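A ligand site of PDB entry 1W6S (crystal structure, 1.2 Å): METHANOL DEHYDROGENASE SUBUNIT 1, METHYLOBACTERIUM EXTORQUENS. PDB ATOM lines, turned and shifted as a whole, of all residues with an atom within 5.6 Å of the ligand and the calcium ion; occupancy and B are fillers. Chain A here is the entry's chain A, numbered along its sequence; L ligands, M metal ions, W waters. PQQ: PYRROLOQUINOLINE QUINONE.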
ATOM      1  N   GLU A  55     -17.014  15.600 -12.614  1.00  0.00           N
ATOM      2  CA  GLU A  55     -16.303  14.410 -12.102  1.00  0.00           C
ATOM      3  C   GLU A  55     -16.170  14.438 -10.577  1.00  0.00           C
ATOM      4  O   GLU A  55     -16.569  15.385  -9.866  1.00  0.00           O
ATOM      5  CB  GLU A  55     -14.904  14.264 -12.792  1.00  0.00           C
ATOM      6  CG  GLU A  55     -14.997  13.816 -14.254  1.00  0.00           C
ATOM      7  CD  GLU A  55     -13.719  13.597 -15.013  1.00  0.00           C
ATOM      8  OE1 GLU A  55     -12.606  13.945 -14.606  1.00  0.00           O
ATOM      9  OE2 GLU A  55     -13.837  13.013 -16.180  1.00  0.00           O
ATOM     10  N   CYS A 103      -6.636  19.008 -22.833  1.00  0.00           N
ATOM     11  CA  CYS A 103      -6.800  17.952 -23.838  1.00  0.00           C
ATOM     12  C   CYS A 103      -8.202  17.370 -23.928  1.00  0.00           C
ATOM     13  O   CYS A 103      -8.584  16.906 -25.043  1.00  0.00           O
ATOM     14  CB  CYS A 103      -5.889  16.707 -23.658  1.00  0.00           C
ATOM     15  SG  CYS A 103      -6.149  15.652 -22.204  1.00  0.00           S
ATOM     16  N   CYS A 104      -8.963  17.248 -22.857  1.00  0.00           N
ATOM     17  CA  CYS A 104      -9.970  16.204 -22.648  1.00  0.00           C
ATOM     18  C   CYS A 104     -11.189  16.672 -21.835  1.00  0.00           C
ATOM     19  O   CYS A 104     -11.708  15.922 -20.946  1.00  0.00           O
ATOM     20  CB  CYS A 104      -9.216  15.103 -21.899  1.00  0.00           C
ATOM     21  SG  CYS A 104      -7.758  14.355 -22.726  1.00  0.00           S
ATOM     22  N   ASP A 105     -11.682  17.873 -22.083  1.00  0.00           N
ATOM     23  CA  ASP A 105     -12.785  18.623 -21.445  1.00  0.00           C
ATOM     24  C   ASP A 105     -12.315  19.423 -20.202  1.00  0.00           C
ATOM     25  O   ASP A 105     -11.212  19.198 -19.643  1.00  0.00           O
ATOM     26  CB  ASP A 105     -13.998  17.744 -21.111  1.00  0.00           C
ATOM     27  CG  ASP A 105     -15.309  18.483 -20.883  1.00  0.00           C
ATOM     28  OD1 ASP A 105     -15.508  19.697 -21.208  1.00  0.00           O
ATOM     29  OD2 ASP A 105     -16.257  17.834 -20.325  1.00  0.00           O
ATOM     30  N   VAL A 107     -12.803  19.474 -16.931  1.00  0.00           N
ATOM     31  CA  VAL A 107     -13.185  18.709 -15.715  1.00  0.00           C
ATOM     32  C   VAL A 107     -12.326  18.997 -14.460  1.00  0.00           C
ATOM     33  O   VAL A 107     -11.189  19.543 -14.574  1.00  0.00           O
ATOM     34  CB  VAL A 107     -13.207  17.195 -16.060  1.00  0.00           C
ATOM     35  CG1 VAL A 107     -14.297  16.852 -17.102  1.00  0.00           C
ATOM     36  CG2 VAL A 107     -11.857  16.665 -16.557  1.00  0.00           C
ATOM     37  N   ARG A 109     -11.614  16.726 -10.416  1.00  0.00           N
ATOM     38  CA  ARG A 109     -11.937  15.474  -9.683  1.00  0.00           C
ATOM     39  C   ARG A 109     -12.211  15.706  -8.201  1.00  0.00           C
ATOM     40  O   ARG A 109     -12.511  14.692  -7.496  1.00  0.00           O
ATOM     41  CB  ARG A 109     -10.847  14.385  -9.967  1.00  0.00           C
ATOM     42  CG  ARG A 109     -10.853  13.964 -11.427  1.00  0.00           C
ATOM     43  CD  ARG A 109      -9.888  12.772 -11.852  1.00  0.00           C
ATOM     44  NE  ARG A 109      -9.932  12.985 -13.323  1.00  0.00           N
ATOM     45  CZ  ARG A 109      -9.181  13.740 -14.071  1.00  0.00           C
ATOM     46  NH1 ARG A 109      -8.096  14.313 -13.554  1.00  0.00           N
ATOM     47  NH2 ARG A 109      -9.504  13.884 -15.358  1.00  0.00           N
ATOM     48  N   THR A 157      -1.632  22.369 -16.987  1.00  0.00           N
ATOM     49  CA  THR A 157      -2.954  22.654 -16.320  1.00  0.00           C
ATOM     50  C   THR A 157      -3.144  21.774 -15.050  1.00  0.00           C
ATOM     51  O   THR A 157      -2.318  20.845 -14.789  1.00  0.00           O
ATOM     52  CB  THR A 157      -4.170  22.441 -17.250  1.00  0.00           C
ATOM     53  OG1 THR A 157      -4.194  21.061 -17.742  1.00  0.00           O
ATOM     54  CG2 THR A 157      -4.207  23.354 -18.473  1.00  0.00           C
ATOM     55  N   THR A 159      -6.319  19.234 -13.192  1.00  0.00           N
ATOM     56  CA  THR A 159      -7.651  18.613 -13.068  1.00  0.00           C
ATOM     57  C   THR A 159      -7.741  17.688 -11.847  1.00  0.00           C
ATOM     58  O   THR A 159      -8.887  17.356 -11.396  1.00  0.00           O
ATOM     59  CB  THR A 159      -8.011  17.845 -14.370  1.00  0.00           C
ATOM     60  OG1 THR A 159      -6.992  16.801 -14.535  1.00  0.00           O
ATOM     61  CG2 THR A 159      -8.044  18.736 -15.618  1.00  0.00           C
ATOM     62  N   SER A 173      -0.265  16.745 -11.542  1.00  0.00           N
ATOM     63  CA  SER A 173       0.131  17.460 -12.813  1.00  0.00           C
ATOM     64  C   SER A 173      -0.609  16.944 -14.054  1.00  0.00           C
ATOM     65  O   SER A 173      -1.043  15.773 -14.008  1.00  0.00           O
ATOM     66  CB  SER A 173       1.659  17.406 -13.039  1.00  0.00           C
ATOM     67  OG  SER A 173       2.181  16.049 -12.962  1.00  0.00           O
ATOM     68  N   SER A 174      -0.804  17.794 -15.090  1.00  0.00           N
ATOM     69  CA  SER A 174      -1.446  17.460 -16.374  1.00  0.00           C
ATOM     70  C   SER A 174      -0.724  18.164 -17.552  1.00  0.00           C
ATOM     71  O   SER A 174      -0.170  19.272 -17.353  1.00  0.00           O
ATOM     72  CB  SER A 174      -2.937  17.848 -16.415  1.00  0.00           C
ATOM     73  OG  SER A 174      -3.735  17.038 -15.534  1.00  0.00           O
ATOM     74  N   GLY A 175      -0.787  17.545 -18.752  1.00  0.00           N
ATOM     75  CA  GLY A 175      -0.254  18.137 -19.991  1.00  0.00           C
ATOM     76  C   GLY A 175       0.703  17.251 -20.805  1.00  0.00           C
ATOM     77  O   GLY A 175       1.442  17.783 -21.669  1.00  0.00           O
ATOM     78  N   ALA A 176       0.719  15.907 -20.675  1.00  0.00           N
ATOM     79  CA  ALA A 176       1.642  15.086 -21.479  1.00  0.00           C
ATOM     80  C   ALA A 176       1.295  15.210 -22.985  1.00  0.00           C
ATOM     81  O   ALA A 176       2.230  15.018 -23.817  1.00  0.00           O
ATOM     82  CB  ALA A 176       1.641  13.614 -21.006  1.00  0.00           C
ATOM     83  N   GLU A 177       0.069  15.537 -23.390  1.00  0.00           N
ATOM     84  CA  GLU A 177      -0.278  15.719 -24.822  1.00  0.00           C
ATOM     85  C   GLU A 177       0.354  16.991 -25.395  1.00  0.00           C
ATOM     86  O   GLU A 177       0.358  17.185 -26.639  1.00  0.00           O
ATOM     87  CB  GLU A 177      -1.814  15.689 -25.041  1.00  0.00           C
ATOM     88  CG  GLU A 177      -2.417  14.269 -25.186  1.00  0.00           C
ATOM     89  CD  GLU A 177      -2.226  13.338 -24.008  1.00  0.00           C
ATOM     90  OE1 GLU A 177      -1.334  12.437 -23.933  1.00  0.00           O
ATOM     91  OE2 GLU A 177      -2.933  13.624 -22.991  1.00  0.00           O
ATOM     92  N   THR A 241       3.103  12.841 -16.358  1.00  0.00           N
ATOM     93  CA  THR A 241       2.213  13.594 -15.454  1.00  0.00           C
ATOM     94  C   THR A 241       1.333  12.655 -14.610  1.00  0.00           C
ATOM     95  O   THR A 241       0.986  11.543 -15.115  1.00  0.00           O
ATOM     96  CB  THR A 241       1.327  14.593 -16.272  1.00  0.00           C
ATOM     97  OG1 THR A 241       0.774  13.859 -17.392  1.00  0.00           O
ATOM     98  CG2 THR A 241       2.152  15.806 -16.760  1.00  0.00           C
ATOM     99  N   TRP A 243      -2.341  12.472 -12.761  1.00  0.00           N
ATOM    100  CA  TRP A 243      -3.647  13.203 -12.677  1.00  0.00           C
ATOM    101  C   TRP A 243      -4.795  12.343 -12.120  1.00  0.00           C
ATOM    102  O   TRP A 243      -5.976  12.780 -12.117  1.00  0.00           O
ATOM    103  CB  TRP A 243      -3.995  13.837 -14.058  1.00  0.00           C
ATOM    104  CG  TRP A 243      -3.868  12.892 -15.243  1.00  0.00           C
ATOM    105  CD1 TRP A 243      -2.713  12.660 -15.952  1.00  0.00           C
ATOM    106  CD2 TRP A 243      -4.888  12.060 -15.860  1.00  0.00           C
ATOM    107  NE1 TRP A 243      -2.942  11.734 -16.967  1.00  0.00           N
ATOM    108  CE2 TRP A 243      -4.296  11.354 -16.925  1.00  0.00           C
ATOM    109  CE3 TRP A 243      -6.261  11.853 -15.608  1.00  0.00           C
ATOM    110  CZ2 TRP A 243      -5.011  10.462 -17.720  1.00  0.00           C
ATOM    111  CZ3 TRP A 243      -6.995  10.944 -16.419  1.00  0.00           C
ATOM    112  CH2 TRP A 243      -6.357  10.254 -17.491  1.00  0.00           C
ATOM    113  N   ASN A 261       1.724   8.732 -19.402  1.00  0.00           N
ATOM    114  CA  ASN A 261       2.401   8.349 -20.657  1.00  0.00           C
ATOM    115  C   ASN A 261       3.609   9.213 -21.059  1.00  0.00           C
ATOM    116  O   ASN A 261       3.644  10.427 -20.727  1.00  0.00           O
ATOM    117  CB  ASN A 261       1.388   8.377 -21.825  1.00  0.00           C
ATOM    118  CG  ASN A 261       0.688   9.719 -22.038  1.00  0.00           C
ATOM    119  OD1 ASN A 261       0.015  10.261 -21.132  1.00  0.00           O
ATOM    120  ND2 ASN A 261       0.834  10.241 -23.274  1.00  0.00           N
ATOM    121  N   TRP A 265       3.084  10.951 -28.787  1.00  0.00           N
ATOM    122  CA  TRP A 265       2.481   9.617 -29.068  1.00  0.00           C
ATOM    123  C   TRP A 265       3.251   8.857 -30.157  1.00  0.00           C
ATOM    124  O   TRP A 265       3.197   7.612 -30.154  1.00  0.00           O
ATOM    125  CB  TRP A 265       0.990   9.731 -29.418  1.00  0.00           C
ATOM    126  CG  TRP A 265       0.011  10.239 -28.364  1.00  0.00           C
ATOM    127  CD1 TRP A 265       0.272  10.945 -27.214  1.00  0.00           C
ATOM    128  CD2 TRP A 265      -1.431  10.078 -28.379  1.00  0.00           C
ATOM    129  NE1 TRP A 265      -0.880  11.217 -26.536  1.00  0.00           N
ATOM    130  CE2 TRP A 265      -1.968  10.697 -27.226  1.00  0.00           C
ATOM    131  CE3 TRP A 265      -2.354   9.467 -29.257  1.00  0.00           C
ATOM    132  CZ2 TRP A 265      -3.327  10.735 -26.907  1.00  0.00           C
ATOM    133  CZ3 TRP A 265      -3.711   9.508 -28.925  1.00  0.00           C
ATOM    134  CH2 TRP A 265      -4.214  10.141 -27.770  1.00  0.00           C
ATOM    135  N   ASP A 303      -0.542   5.178 -25.940  1.00  0.00           N
ATOM    136  CA  ASP A 303      -1.184   6.095 -24.955  1.00  0.00           C
ATOM    137  C   ASP A 303      -1.867   5.346 -23.799  1.00  0.00           C
ATOM    138  O   ASP A 303      -3.021   5.713 -23.405  1.00  0.00           O
ATOM    139  CB  ASP A 303      -2.145   7.111 -25.633  1.00  0.00           C
ATOM    140  CG  ASP A 303      -2.736   8.136 -24.713  1.00  0.00           C
ATOM    141  OD1 ASP A 303      -2.077   8.685 -23.814  1.00  0.00           O
ATOM    142  OD2 ASP A 303      -3.949   8.462 -24.828  1.00  0.00           O
ATOM    143  N   ALA A 305      -1.857   5.662 -20.497  1.00  0.00           N
ATOM    144  CA  ALA A 305      -1.438   6.443 -19.312  1.00  0.00           C
ATOM    145  C   ALA A 305      -1.670   5.793 -17.945  1.00  0.00           C
ATOM    146  O   ALA A 305      -2.803   5.449 -17.550  1.00  0.00           O
ATOM    147  CB  ALA A 305      -2.098   7.849 -19.374  1.00  0.00           C
ATOM    148  N   ARG A 331      -4.965   1.031 -17.726  1.00  0.00           N
ATOM    149  CA  ARG A 331      -5.356   1.318 -19.113  1.00  0.00           C
ATOM    150  C   ARG A 331      -4.966   0.188 -20.095  1.00  0.00           C
ATOM    151  O   ARG A 331      -5.697  -0.091 -21.049  1.00  0.00           O
ATOM    152  CB  ARG A 331      -4.785   2.658 -19.637  1.00  0.00           C
ATOM    153  CG  ARG A 331      -5.382   3.960 -19.034  1.00  0.00           C
ATOM    154  CD  ARG A 331      -6.367   4.616 -19.984  1.00  0.00           C
ATOM    155  NE  ARG A 331      -5.844   5.484 -21.017  1.00  0.00           N
ATOM    156  CZ  ARG A 331      -5.554   6.795 -20.960  1.00  0.00           C
ATOM    157  NH1 ARG A 331      -5.717   7.489 -19.824  1.00  0.00           N
ATOM    158  NH2 ARG A 331      -5.079   7.445 -22.047  1.00  0.00           N
ATOM    159  N   ALA A 389      -6.542   3.386 -27.015  1.00  0.00           N
ATOM    160  CA  ALA A 389      -5.939   4.422 -26.157  1.00  0.00           C
ATOM    161  C   ALA A 389      -6.872   4.890 -25.047  1.00  0.00           C
ATOM    162  O   ALA A 389      -6.387   5.384 -24.012  1.00  0.00           O
ATOM    163  CB  ALA A 389      -5.524   5.604 -27.048  1.00  0.00           C
ATOM    164  N   MET A 390      -8.210   4.796 -25.187  1.00  0.00           N
ATOM    165  CA  MET A 390      -9.149   5.123 -24.102  1.00  0.00           C
ATOM    166  C   MET A 390      -9.053   4.099 -22.954  1.00  0.00           C
ATOM    167  O   MET A 390      -9.563   4.336 -21.810  1.00  0.00           O
ATOM    168  CB  MET A 390     -10.586   5.245 -24.647  1.00  0.00           C
ATOM    169  CG  MET A 390     -10.772   6.352 -25.677  1.00  0.00           C
ATOM    170  SD  MET A 390     -12.444   6.690 -26.289  1.00  0.00           S
ATOM    171  CE  MET A 390     -13.030   7.807 -24.946  1.00  0.00           C
ATOM    172  N   ASN A 394     -10.340   3.543 -17.334  1.00  0.00           N
ATOM    173  CA  ASN A 394      -9.801   4.956 -17.328  1.00  0.00           C
ATOM    174  C   ASN A 394      -9.926   5.496 -15.891  1.00  0.00           C
ATOM    175  O   ASN A 394      -9.713   4.758 -14.904  1.00  0.00           O
ATOM    176  CB  ASN A 394     -10.413   5.783 -18.441  1.00  0.00           C
ATOM    177  CG  ASN A 394      -9.695   7.013 -18.953  1.00  0.00           C
ATOM    178  OD1 ASN A 394      -9.113   7.114 -20.092  1.00  0.00           O
ATOM    179  ND2 ASN A 394      -9.612   8.086 -18.214  1.00  0.00           N
ATOM    180  N   GLN A 395     -10.236   6.760 -15.608  1.00  0.00           N
ATOM    181  CA  GLN A 395     -10.160   7.530 -14.371  1.00  0.00           C
ATOM    182  C   GLN A 395     -11.244   7.192 -13.305  1.00  0.00           C
ATOM    183  O   GLN A 395     -11.232   7.849 -12.226  1.00  0.00           O
ATOM    184  CB  GLN A 395     -10.218   9.078 -14.630  1.00  0.00           C
ATOM    185  CG  GLN A 395     -11.489   9.547 -15.348  1.00  0.00           C
ATOM    186  CD  GLN A 395     -12.654   9.937 -14.456  1.00  0.00           C
ATOM    187  OE1 GLN A 395     -13.816   9.419 -14.572  1.00  0.00           O
ATOM    188  NE2 GLN A 395     -12.408  10.853 -13.527  1.00  0.00           N
ATOM    189  N   TRP A 476     -17.605   4.725 -16.940  1.00  0.00           N
ATOM    190  CA  TRP A 476     -16.513   5.686 -16.838  1.00  0.00           C
ATOM    191  C   TRP A 476     -16.241   6.245 -15.431  1.00  0.00           C
ATOM    192  O   TRP A 476     -15.093   6.683 -15.150  1.00  0.00           O
ATOM    193  CB  TRP A 476     -16.789   6.882 -17.815  1.00  0.00           C
ATOM    194  CG  TRP A 476     -15.568   7.669 -18.281  1.00  0.00           C
ATOM    195  CD1 TRP A 476     -15.169   8.906 -17.823  1.00  0.00           C
ATOM    196  CD2 TRP A 476     -14.582   7.317 -19.292  1.00  0.00           C
ATOM    197  NE1 TRP A 476     -14.012   9.322 -18.476  1.00  0.00           N
ATOM    198  CE2 TRP A 476     -13.636   8.344 -19.397  1.00  0.00           C
ATOM    199  CE3 TRP A 476     -14.425   6.196 -20.148  1.00  0.00           C
ATOM    200  CZ2 TRP A 476     -12.552   8.278 -20.306  1.00  0.00           C
ATOM    201  CZ3 TRP A 476     -13.373   6.096 -21.038  1.00  0.00           C
ATOM    202  CH2 TRP A 476     -12.454   7.150 -21.112  1.00  0.00           C
ATOM    203  N   GLY A 538     -19.548  14.463 -20.058  1.00  0.00           N
ATOM    204  CA  GLY A 538     -18.355  15.138 -20.591  1.00  0.00           C
ATOM    205  C   GLY A 538     -17.119  14.272 -20.479  1.00  0.00           C
ATOM    206  O   GLY A 538     -17.202  13.031 -20.627  1.00  0.00           O
ATOM    207  N   GLY A 539     -15.943  14.893 -20.191  1.00  0.00           N
ATOM    208  CA  GLY A 539     -14.696  14.119 -20.210  1.00  0.00           C
ATOM    209  C   GLY A 539     -14.351  13.654 -21.637  1.00  0.00           C
ATOM    210  O   GLY A 539     -15.003  14.147 -22.577  1.00  0.00           O
ATOM    211  N   TRP A 540     -13.402  12.712 -21.790  1.00  0.00           N
ATOM    212  CA  TRP A 540     -13.033  12.252 -23.141  1.00  0.00           C
ATOM    213  C   TRP A 540     -14.236  11.681 -23.897  1.00  0.00           C
ATOM    214  O   TRP A 540     -14.411  12.081 -25.108  1.00  0.00           O
ATOM    215  CB  TRP A 540     -11.824  11.274 -23.096  1.00  0.00           C
ATOM    216  CG  TRP A 540     -11.035  11.096 -24.370  1.00  0.00           C
ATOM    217  CD1 TRP A 540     -11.259  11.718 -25.577  1.00  0.00           C
ATOM    218  CD2 TRP A 540      -9.884  10.245 -24.589  1.00  0.00           C
ATOM    219  NE1 TRP A 540     -10.314  11.308 -26.542  1.00  0.00           N
ATOM    220  CE2 TRP A 540      -9.460  10.393 -25.944  1.00  0.00           C
ATOM    221  CE3 TRP A 540      -9.156   9.357 -23.762  1.00  0.00           C
ATOM    222  CZ2 TRP A 540      -8.364   9.695 -26.463  1.00  0.00           C
ATOM    223  CZ3 TRP A 540      -8.055   8.653 -24.287  1.00  0.00           C
ATOM    224  CH2 TRP A 540      -7.670   8.834 -25.624  1.00  0.00           C
ATOM    225  N   PRO A 541     -15.121  10.801 -23.386  1.00  0.00           N
ATOM    226  CA  PRO A 541     -16.254  10.267 -24.192  1.00  0.00           C
ATOM    227  C   PRO A 541     -17.269  11.284 -24.683  1.00  0.00           C
ATOM    228  O   PRO A 541     -17.910  11.102 -25.740  1.00  0.00           O
ATOM    229  CB  PRO A 541     -16.960   9.284 -23.213  1.00  0.00           C
ATOM    230  CG  PRO A 541     -15.983   9.005 -22.094  1.00  0.00           C
ATOM    231  CD  PRO A 541     -15.093  10.221 -22.020  1.00  0.00           C
HETATM  232  N1  PQQ L   1      -8.953  13.163 -18.737  1.00  0.00           N
HETATM  233  C2  PQQ L   1     -10.058  12.214 -19.138  1.00  0.00           C
HETATM  234  C2X PQQ L   1     -11.417  12.444 -18.579  1.00  0.00           C
HETATM  235  O2A PQQ L   1     -11.598  13.281 -17.642  1.00  0.00           O
HETATM  236  O2B PQQ L   1     -12.394  11.726 -19.087  1.00  0.00           O
HETATM  237  C3  PQQ L   1      -9.546  11.188 -20.030  1.00  0.00           C
HETATM  238  C3A PQQ L   1      -8.160  11.531 -20.168  1.00  0.00           C
HETATM  239  C1A PQQ L   1      -7.787  12.772 -19.411  1.00  0.00           C
HETATM  240  C4  PQQ L   1      -7.133  10.772 -20.893  1.00  0.00           C
HETATM  241  O4  PQQ L   1      -7.388   9.577 -21.423  1.00  0.00           O
HETATM  242  C5  PQQ L   1      -5.896  11.239 -20.996  1.00  0.00           C
HETATM  243  O5  PQQ L   1      -4.749  10.560 -21.458  1.00  0.00           O
HETATM  244  C6A PQQ L   1      -5.472  12.467 -20.247  1.00  0.00           C
HETATM  245  N6  PQQ L   1      -4.112  12.717 -20.159  1.00  0.00           N
HETATM  246  C7  PQQ L   1      -3.571  13.813 -19.418  1.00  0.00           C
HETATM  247  C7X PQQ L   1      -2.066  13.909 -19.481  1.00  0.00           C
HETATM  248  O7A PQQ L   1      -1.507  13.143 -20.261  1.00  0.00           O
HETATM  249  O7B PQQ L   1      -1.516  14.780 -18.807  1.00  0.00           O
HETATM  250  C8  PQQ L   1      -4.487  14.639 -18.674  1.00  0.00           C
HETATM  251  C9  PQQ L   1      -5.936  14.417 -18.566  1.00  0.00           C
HETATM  252  C9X PQQ L   1      -6.711  15.287 -17.588  1.00  0.00           C
HETATM  253  O9A PQQ L   1      -5.974  16.168 -16.953  1.00  0.00           O
HETATM  254  O9B PQQ L   1      -7.965  15.215 -17.493  1.00  0.00           O
HETATM  255  C9A PQQ L   1      -6.430  13.242 -19.387  1.00  0.00           C
HETATM  256 CA    CA M   1      -2.777  11.619 -21.689  1.00  0.00          CA
HETATM  257  O   HOH W   1      -0.224  11.225 -18.430  1.00  0.00           O
HETATM  258  O   HOH W   2      -5.960  18.938 -18.748  1.00  0.00           O
HETATM  259  O   HOH W   3      -2.497  16.125 -21.761  1.00  0.00           O
HETATM  260  O   HOH W   4      -5.270  10.740 -24.068  1.00  0.00           O
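The calcium ion is bound by an oxygen (O5) of the ligand (2.3 Å), a nitrogen (N6) of the ligand (2.3 Å), the side-chain carboxylate (OE2) of Glu 177 (2.4 Å), an oxygen (O7A) of the ligand (2.4 Å) and the side-chain carboxylate (OE1) of Glu 177 (2.8 Å). The calcium ion has five donor atoms within binding distance.
O2B of the ligand is in hydrogen-bond range of NE1 of Trp 476, at 3.0 Å. The backbone NH of Gly 175 lies within hydrogen-bond range of an oxygen (O7B) of the ligand, at 2.9 Å. The guanidinium group (NH1) of Arg 331 lies within hydrogen-bond range of an oxygen (O4) of the ligand (3.1 Å). N of Ala 176 is in hydrogen-bond range of O7B of the ligand (3.1 Å). The side-chain hydroxyl (OG1) of Thr 241 sits at hydrogen-bond distance from an oxygen (O7B) of the ligand, at 2.8 Å. O2A of the ligand lies close to OE2 of Glu 55 (2.7 Å). The side-chain amide oxygen (OD1) of Asn 261 sits close to an oxygen (O7A) of the ligand (3.4 Å). The guanidinium group of Arg 109 lies within salt-bridge range of an oxygen (O9B) of the ligand, at 2.9 Å. The backbone NH of Trp 540 sits at hydrogen-bond distance from an oxygen (O2B) of the ligand, at 3.0 Å. O4 of the ligand sits close to OD1 of Asn 394, at 3.3 Å. The side-chain hydroxyl (OG1) of Thr 159 is in hydrogen-bond range of an oxygen (O9A) of the ligand, 2.7 Å away. The side-chain hydroxyl (OG) of Ser 174 is in hydrogen-bond range of an oxygen (O9A) of the ligand (2.8 Å).
Water W1 lies within hydrogen-bond range of the side-chain amide oxygen (OD1) of Asn 261 (2.9 Å), the side-chain hydroxyl (OG1) of Thr 241 (3.0 Å) and the indole nitrogen (NE1) of Trp 243 (3.1 Å). Water W3 lies within hydrogen-bond range of the backbone NH of Glu 177 (3.1 Å), an oxygen (O7B) of the ligand (3.4 Å), the backbone NH of Ala 176 (3.4 Å) and the side-chain sulfur of Cys 103 (3.7 Å). Water W2 lies within hydrogen-bond range of OG1 of Thr 157 and O9A of the ligand.
Cys 103 touches the ligand. Cys 104 touches the ligand (SG to C1A, 3.7 Å). Val 107 touches the ligand (CG2 to O2A, 3.6 Å). Trp 243 touches the ligand (CZ2 to C6A, 3.3 Å). CA of Gly 539 touches O2B of the ligand, 3.5 Å away. Of the 29 residues printed, 18 come within 4 Å of the ligand. The nearest printed residue that does not touch the ligand is Asp 303 (4.03 Å).
The backbone carbonyl oxygen (O) of Trp 476 lies close to the side-chain amide oxygen (OE1) of Gln 395, at 3.1 Å. The side-chain hydroxyl of Thr 159 is in hydrogen-bond range of the guanidinium group of Arg 109 (2.9 Å). OE1 of Glu 177 sits close to NE1 of Trp 265 (2.9 Å). OD2 of Asp 303 lies within salt-bridge range of NH2 of Arg 331 (3.2 Å). The side-chain amide oxygen (OD1) of Asn 394 lies close to the backbone carbonyl oxygen (O) of Met 390 (3.3 Å). OE1 of Glu 55 is in salt-bridge range of NE of Arg 109 (3.1 Å). OG of Ser 174 lies within hydrogen-bond range of OG1 of Thr 159 (3.4 Å). NE of Arg 331 sits at hydrogen-bond distance from O of Ala 389 (3.0 Å).
Merely in contact with the calcium ion: Asn 261 (3.2 Å) and Asp 303 (3.7 Å). The nearest printed residue that does not touch the calcium ion is Ala 305 (4.5 Å).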
